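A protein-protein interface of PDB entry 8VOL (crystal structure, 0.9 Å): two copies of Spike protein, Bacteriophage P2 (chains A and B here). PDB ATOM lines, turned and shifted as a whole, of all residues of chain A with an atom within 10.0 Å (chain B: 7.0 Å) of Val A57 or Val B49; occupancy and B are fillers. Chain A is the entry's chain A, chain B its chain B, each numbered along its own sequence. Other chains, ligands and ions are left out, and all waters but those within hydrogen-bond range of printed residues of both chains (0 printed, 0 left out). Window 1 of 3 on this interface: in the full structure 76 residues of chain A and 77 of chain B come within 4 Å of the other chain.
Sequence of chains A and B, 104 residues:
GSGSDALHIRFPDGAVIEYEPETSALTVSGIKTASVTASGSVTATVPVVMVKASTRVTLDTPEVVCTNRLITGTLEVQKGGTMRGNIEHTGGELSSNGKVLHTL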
ATOM      1  N   LYS A  32       0.799 -36.309  22.086  1.00  0.00           N
ATOM      2  CA  LYS A  32       0.719 -36.899  20.755  1.00  0.00           C
ATOM      3  C   LYS A  32      -0.367 -36.241  19.915  1.00  0.00           C
ATOM      4  O   LYS A  32      -0.107 -35.837  18.778  1.00  0.00           O
ATOM      5  CB  LYS A  32       0.503 -38.416  20.825  1.00  0.00           C
ATOM      6  CG  LYS A  32       0.529 -39.090  19.479  1.00  0.00           C
ATOM      7  CD  LYS A  32       0.920 -40.550  19.529  1.00  0.00           C
ATOM      8  CE  LYS A  32      -0.049 -41.399  20.282  1.00  0.00           C
ATOM      9  NZ  LYS A  32       0.455 -42.803  20.352  1.00  0.00           N
ATOM     10  N   ALA A  34      -3.902 -33.439  19.967  1.00  0.00           N
ATOM     11  CA  ALA A  34      -4.899 -32.574  20.566  1.00  0.00           C
ATOM     12  C   ALA A  34      -6.099 -32.509  19.634  1.00  0.00           C
ATOM     13  O   ALA A  34      -5.956 -32.529  18.400  1.00  0.00           O
ATOM     14  CB  ALA A  34      -4.373 -31.157  20.807  1.00  0.00           C
ATOM     15  N   VAL A  49       1.450 -15.637  13.957  1.00  0.00           N
ATOM     16  CA  VAL A  49       1.088 -17.046  14.061  1.00  0.00           C
ATOM     17  C   VAL A  49       2.108 -17.839  13.268  1.00  0.00           C
ATOM     18  O   VAL A  49       2.398 -17.502  12.113  1.00  0.00           O
ATOM     19  CB  VAL A  49      -0.334 -17.308  13.529  1.00  0.00           C
ATOM     20  CG1 VAL A  49      -0.640 -18.788  13.487  1.00  0.00           C
ATOM     21  CG2 VAL A  49      -1.327 -16.564  14.381  1.00  0.00           C
ATOM     22  N   MET A  50       2.636 -18.894  13.877  1.00  0.00           N
ATOM     23  CA  MET A  50       3.618 -19.767  13.250  1.00  0.00           C
ATOM     24  C   MET A  50       3.127 -21.199  13.380  1.00  0.00           C
ATOM     25  O   MET A  50       2.940 -21.683  14.495  1.00  0.00           O
ATOM     26  CB  MET A  50       4.975 -19.624  13.958  1.00  0.00           C
ATOM     27  CG  MET A  50       6.065 -20.577  13.496  1.00  0.00           C
ATOM     28  SD  MET A  50       6.368 -20.504  11.721  1.00  0.00           S
ATOM     29  CE  MET A  50       7.184 -18.915  11.621  1.00  0.00           C
ATOM     30  N   VAL A  51       2.938 -21.874  12.254  1.00  0.00           N
ATOM     31  CA  VAL A  51       2.572 -23.283  12.234  1.00  0.00           C
ATOM     32  C   VAL A  51       3.721 -24.023  11.569  1.00  0.00           C
ATOM     33  O   VAL A  51       3.998 -23.811  10.385  1.00  0.00           O
ATOM     34  CB  VAL A  51       1.251 -23.511  11.495  1.00  0.00           C
ATOM     35  CG1 VAL A  51       0.916 -24.990  11.481  1.00  0.00           C
ATOM     36  CG2 VAL A  51       0.137 -22.695  12.119  1.00  0.00           C
ATOM     37  N   LYS A  52       4.407 -24.867  12.334  1.00  0.00           N
ATOM     38  CA  LYS A  52       5.556 -25.634  11.866  1.00  0.00           C
ATOM     39  C   LYS A  52       5.088 -27.079  11.792  1.00  0.00           C
ATOM     40  O   LYS A  52       5.027 -27.771  12.814  1.00  0.00           O
ATOM     41  CB  LYS A  52       6.736 -25.442  12.813  1.00  0.00           C
ATOM     42  CG  LYS A  52       8.026 -26.127  12.430  1.00  0.00           C
ATOM     43  CD  LYS A  52       8.573 -25.616  11.118  1.00  0.00           C
ATOM     44  CE  LYS A  52       9.974 -26.143  10.837  1.00  0.00           C
ATOM     45  NZ  LYS A  52      10.478 -25.803   9.490  1.00  0.00           N
ATOM     46  N   ALA A  53       4.703 -27.520  10.592  1.00  0.00           N
ATOM     47  CA  ALA A  53       4.022 -28.800  10.402  1.00  0.00           C
ATOM     48  C   ALA A  53       4.788 -29.620   9.368  1.00  0.00           C
ATOM     49  O   ALA A  53       4.666 -29.405   8.158  1.00  0.00           O
ATOM     50  CB  ALA A  53       2.582 -28.597   9.980  1.00  0.00           C
ATOM     51  N   SER A  54       5.569 -30.585   9.842  1.00  0.00           N
ATOM     52  CA  SER A  54       6.487 -31.294   8.968  1.00  0.00           C
ATOM     53  C   SER A  54       5.796 -32.191   7.941  1.00  0.00           C
ATOM     54  O   SER A  54       6.462 -32.610   6.985  1.00  0.00           O
ATOM     55  CB  SER A  54       7.477 -32.101   9.801  1.00  0.00           C
ATOM     56  OG  SER A  54       6.809 -33.038  10.616  1.00  0.00           O
ATOM     57  N   THR A  55       4.509 -32.513   8.121  1.00  0.00           N
ATOM     58  CA  THR A  55       3.765 -33.259   7.111  1.00  0.00           C
ATOM     59  C   THR A  55       2.874 -32.332   6.277  1.00  0.00           C
ATOM     60  O   THR A  55       3.104 -32.188   5.069  1.00  0.00           O
ATOM     61  CB  THR A  55       2.972 -34.413   7.717  1.00  0.00           C
ATOM     62  OG1 THR A  55       3.885 -35.299   8.372  1.00  0.00           O
ATOM     63  CG2 THR A  55       2.213 -35.185   6.637  1.00  0.00           C
ATOM     64  N   ARG A  56       1.851 -31.723   6.885  1.00  0.00           N
ATOM     65  CA  ARG A  56       0.838 -31.028   6.094  1.00  0.00           C
ATOM     66  C   ARG A  56      -0.112 -30.269   7.005  1.00  0.00           C
ATOM     67  O   ARG A  56      -0.486 -30.751   8.081  1.00  0.00           O
ATOM     68  CB  ARG A  56       0.022 -32.049   5.290  1.00  0.00           C
ATOM     69  CG  ARG A  56      -1.081 -31.481   4.401  1.00  0.00           C
ATOM     70  CD  ARG A  56      -1.714 -32.572   3.557  1.00  0.00           C
ATOM     71  NE  ARG A  56      -0.773 -33.126   2.586  1.00  0.00           N
ATOM     72  CZ  ARG A  56      -0.116 -34.272   2.718  1.00  0.00           C
ATOM     73  NH1 ARG A  56      -0.245 -35.033   3.797  1.00  0.00           N
ATOM     74  NH2 ARG A  56       0.703 -34.657   1.745  1.00  0.00           N
ATOM     75  N   VAL A  57      -0.560 -29.115   6.508  1.00  0.00           N
ATOM     76  CA  VAL A  57      -1.663 -28.362   7.086  1.00  0.00           C
ATOM     77  C   VAL A  57      -2.851 -28.497   6.143  1.00  0.00           C
ATOM     78  O   VAL A  57      -2.757 -28.092   4.980  1.00  0.00           O
ATOM     79  CB  VAL A  57      -1.299 -26.881   7.258  1.00  0.00           C
ATOM     80  CG1 VAL A  57      -2.500 -26.087   7.768  1.00  0.00           C
ATOM     81  CG2 VAL A  57      -0.095 -26.721   8.173  1.00  0.00           C
ATOM     82  N   THR A  58      -3.979 -29.027   6.649  1.00  0.00           N
ATOM     83  CA  THR A  58      -5.205 -29.150   5.866  1.00  0.00           C
ATOM     84  C   THR A  58      -6.267 -28.227   6.447  1.00  0.00           C
ATOM     85  O   THR A  58      -6.590 -28.308   7.634  1.00  0.00           O
ATOM     86  CB  THR A  58      -5.710 -30.588   5.847  1.00  0.00           C
ATOM     87  OG1 THR A  58      -4.723 -31.440   5.272  1.00  0.00           O
ATOM     88  CG2 THR A  58      -6.986 -30.704   5.023  1.00  0.00           C
ATOM     89  N   LEU A  59      -6.799 -27.364   5.580  1.00  0.00           N
ATOM     90  CA  LEU A  59      -7.903 -26.467   5.876  1.00  0.00           C
ATOM     91  C   LEU A  59      -9.102 -27.021   5.113  1.00  0.00           C
ATOM     92  O   LEU A  59      -9.290 -26.760   3.922  1.00  0.00           O
ATOM     93  CB  LEU A  59      -7.549 -25.049   5.475  1.00  0.00           C
ATOM     94  CG  LEU A  59      -6.256 -24.509   6.081  1.00  0.00           C
ATOM     95  CD1 LEU A  59      -5.998 -23.067   5.597  1.00  0.00           C
ATOM     96  CD2 LEU A  59      -6.254 -24.561   7.614  1.00  0.00           C
ATOM     97  N   ASP A  60      -9.883 -27.851   5.817  1.00  0.00           N
ATOM     98  CA  ASP A  60     -11.002 -28.573   5.213  1.00  0.00           C
ATOM     99  C   ASP A  60     -12.268 -27.793   5.520  1.00  0.00           C
ATOM    100  O   ASP A  60     -12.886 -27.935   6.583  1.00  0.00           O
ATOM    101  CB  ASP A  60     -11.068 -30.002   5.713  1.00  0.00           C
ATOM    102  CG  ASP A  60     -12.199 -30.775   5.089  1.00  0.00           C
ATOM    103  OD1 ASP A  60     -12.570 -31.821   5.647  1.00  0.00           O
ATOM    104  OD2 ASP A  60     -12.779 -30.298   4.087  1.00  0.00           O
ATOM    105  N   THR A  61     -12.634 -26.924   4.581  1.00  0.00           N
ATOM    106  CA  THR A  61     -13.665 -25.928   4.785  1.00  0.00           C
ATOM    107  C   THR A  61     -14.212 -25.535   3.421  1.00  0.00           C
ATOM    108  O   THR A  61     -13.486 -25.604   2.425  1.00  0.00           O
ATOM    109  CB  THR A  61     -13.069 -24.712   5.527  1.00  0.00           C
ATOM    110  OG1 THR A  61     -14.070 -23.741   5.797  1.00  0.00           O
ATOM    111  CG2 THR A  61     -11.941 -24.037   4.760  1.00  0.00           C
ATOM    112  N   VAL A  64     -11.573 -20.802   2.480  1.00  0.00           N
ATOM    113  CA  VAL A  64     -10.471 -20.160   3.185  1.00  0.00           C
ATOM    114  C   VAL A  64     -10.351 -18.750   2.628  1.00  0.00           C
ATOM    115  O   VAL A  64     -10.277 -18.574   1.410  1.00  0.00           O
ATOM    116  CB  VAL A  64      -9.147 -20.909   2.977  1.00  0.00           C
ATOM    117  CG1 VAL A  64      -7.997 -20.165   3.643  1.00  0.00           C
ATOM    118  CG2 VAL A  64      -9.241 -22.331   3.474  1.00  0.00           C
ATOM    119  N   ALA B  44       2.357 -23.489  16.744  1.00  0.00           N
ATOM    120  CA  ALA B  44       2.011 -24.902  16.822  1.00  0.00           C
ATOM    121  C   ALA B  44       3.054 -25.679  16.044  1.00  0.00           C
ATOM    122  O   ALA B  44       3.311 -25.354  14.877  1.00  0.00           O
ATOM    123  CB  ALA B  44       0.621 -25.160  16.231  1.00  0.00           C
ATOM    124  N   THR B  45       3.641 -26.696  16.668  1.00  0.00           N
ATOM    125  CA  THR B  45       4.687 -27.516  16.068  1.00  0.00           C
ATOM    126  C   THR B  45       4.251 -28.971  16.176  1.00  0.00           C
ATOM    127  O   THR B  45       4.270 -29.542  17.270  1.00  0.00           O
ATOM    128  CB  THR B  45       6.032 -27.300  16.759  1.00  0.00           C
ATOM    129  OG1 THR B  45       6.352 -25.907  16.742  1.00  0.00           O
ATOM    130  CG2 THR B  45       7.124 -28.060  16.054  1.00  0.00           C
ATOM    131  N   VAL B  46       3.836 -29.551  15.050  1.00  0.00           N
ATOM    132  CA  VAL B  46       3.179 -30.860  15.043  1.00  0.00           C
ATOM    133  C   VAL B  46       3.165 -31.311  13.587  1.00  0.00           C
ATOM    134  O   VAL B  46       2.971 -30.466  12.703  1.00  0.00           O
ATOM    135  CB  VAL B  46       1.754 -30.772  15.625  1.00  0.00           C
ATOM    136  CG1 VAL B  46       0.910 -29.726  14.925  1.00  0.00           C
ATOM    137  CG2 VAL B  46       1.077 -32.140  15.600  1.00  0.00           C
ATOM    138  N   PRO B  47       3.318 -32.603  13.276  1.00  0.00           N
ATOM    139  CA  PRO B  47       3.429 -32.942  11.843  1.00  0.00           C
ATOM    140  C   PRO B  47       2.186 -32.605  11.037  1.00  0.00           C
ATOM    141  O   PRO B  47       2.300 -32.149   9.894  1.00  0.00           O
ATOM    142  CB  PRO B  47       3.737 -34.439  11.858  1.00  0.00           C
ATOM    143  CG  PRO B  47       4.505 -34.627  13.157  1.00  0.00           C
ATOM    144  CD  PRO B  47       3.746 -33.741  14.136  1.00  0.00           C
ATOM    145  N   VAL B  48       1.005 -32.881  11.593  1.00  0.00           N
ATOM    146  CA  VAL B  48      -0.281 -32.737  10.925  1.00  0.00           C
ATOM    147  C   VAL B  48      -1.128 -31.732  11.681  1.00  0.00           C
ATOM    148  O   VAL B  48      -1.356 -31.881  12.890  1.00  0.00           O
ATOM    149  CB  VAL B  48      -1.005 -34.093  10.824  1.00  0.00           C
ATOM    150  CG1 VAL B  48      -2.473 -33.908  10.445  1.00  0.00           C
ATOM    151  CG2 VAL B  48      -0.295 -34.985   9.838  1.00  0.00           C
ATOM    152  N   VAL B  49      -1.619 -30.720  10.959  1.00  0.00           N
ATOM    153  CA  VAL B  49      -2.647 -29.815  11.452  1.00  0.00           C
ATOM    154  C   VAL B  49      -3.882 -30.019  10.587  1.00  0.00           C
ATOM    155  O   VAL B  49      -3.795 -29.920   9.360  1.00  0.00           O
ATOM    156  CB  VAL B  49      -2.185 -28.352  11.403  1.00  0.00           C
ATOM    157  CG1 VAL B  49      -3.313 -27.418  11.769  1.00  0.00           C
ATOM    158  CG2 VAL B  49      -0.975 -28.160  12.298  1.00  0.00           C
ATOM    159  N   MET B  50      -5.019 -30.304  11.228  1.00  0.00           N
ATOM    160  CA  MET B  50      -6.273 -30.582  10.541  1.00  0.00           C
ATOM    161  C   MET B  50      -7.322 -29.626  11.074  1.00  0.00           C
ATOM    162  O   MET B  50      -7.658 -29.663  12.259  1.00  0.00           O
ATOM    163  CB  MET B  50      -6.684 -32.041  10.772  1.00  0.00           C
ATOM    164  CG  MET B  50      -8.056 -32.342  10.188  1.00  0.00           C
ATOM    165  SD  MET B  50      -8.127 -32.137   8.375  1.00  0.00           S
ATOM    166  CE  MET B  50      -6.861 -33.248   7.836  1.00  0.00           C
ATOM    167  N   VAL B  51      -7.873 -28.793  10.200  1.00  0.00           N
ATOM    168  CA  VAL B  51      -8.935 -27.872  10.562  1.00  0.00           C
ATOM    169  C   VAL B  51     -10.168 -28.268   9.765  1.00  0.00           C
ATOM    170  O   VAL B  51     -10.150 -28.232   8.532  1.00  0.00           O
ATOM    171  CB  VAL B  51      -8.541 -26.414  10.287  1.00  0.00           C
ATOM    172  CG1 VAL B  51      -9.679 -25.483  10.627  1.00  0.00           C
ATOM    173  CG2 VAL B  51      -7.295 -26.054  11.061  1.00  0.00           C
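CG2 of Val B49 touches CG1 of Val A51, 3.8 Å away.
O of Lys A52 touches CA of Thr B45, at 3.3 Å.
CB of Ala A53 touches O of Pro B47, at 3.6 Å.
Val B46 touches Ser A54 (O to N, 3.9 Å).
Pro B47 touches Ser A54 (CA to OG, 3.6 Å).
Thr A55 touches Val B48 (CB to CG2, 3.9 Å).
Val B48 touches Arg A56.
Val A57 touches Val B49 (CA to O, 3.5 Å).
Met B50 touches Thr A58 (CE to CB, 3.5 Å).
Val B51 touches Leu A59.
Printed residues of chain B within 4 Å of Val A51: Ala B44 (3.4 Å) and Val B49 (3.8 Å).
Printed residues of chain B within 4 Å of Ser A54: Val B46 (3.9 Å) and Pro B47 (3.6 Å).
Printed residues of chain B within 4 Å of Arg A56: Pro B47 (3.1 Å), Val B48 (3.5 Å) and Val B49 (3.1 Å).
Val A57 touches just one residue of chain B: Val B49 (3.5 Å).
Val B46 touches just these residues of chain A: Lys A52, Ala A53 and Ser A54.
Val B48 touches just these residues of chain A: Thr A55 (3.9 Å) and Arg A56 (3.5 Å).
Of chain A, only Thr A58 (3.5 Å) comes within 4 Å of Met B50.
Printed residues of chain A within 4 Å of Val B51: Thr A58 (2.9 Å), Leu A59 (3.8 Å) and Asp A60 (2.8 Å).
The nearest residue of chain B that does not touch Val A57 is Pro B47 (5.4 Å).
O of Met A50 sits at hydrogen-bond distance from N of Ala B44, 2.9 Å away.
The backbone NH (N) of Lys A52 is in hydrogen-bond range of the backbone carbonyl oxygen (O) of Ala B44.
O of Lys A52 is in hydrogen-bond range of N of Val B46 (3.1 Å).
The backbone NH (N) of Thr A55 sits at hydrogen-bond distance from the backbone carbonyl oxygen (O) of Pro B47 (2.9 Å).
The backbone NH of Arg A56 sits at hydrogen-bond distance from the backbone carbonyl oxygen of Pro B47 (3.1 Å).
N of Val B49 lies within hydrogen-bond range of O of Arg A56, 3.1 Å away.
The backbone carbonyl oxygen (O) of Val B49 is in hydrogen-bond range of the backbone NH (N) of Thr A58 (2.9 Å).
N of Val B51 lies within hydrogen-bond range of O of Thr A58 (2.9 Å).
The backbone NH (N) of Asp A60 lies within hydrogen-bond range of the backbone carbonyl oxygen (O) of Val B51 (2.8 Å).
Of the 8 printed residues of chain B, 8 touch a printed residue of chain A.
Among the printed residues, no Asp or Glu carboxylate lies within 4 Å of a Lys or Arg side-chain nitrogen of the other chain.
Val A51 touches Val B49, but with the chains exchanged Val A49 does not touch Val B51 (10.1 Å).
3 positions are printed for both chains.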
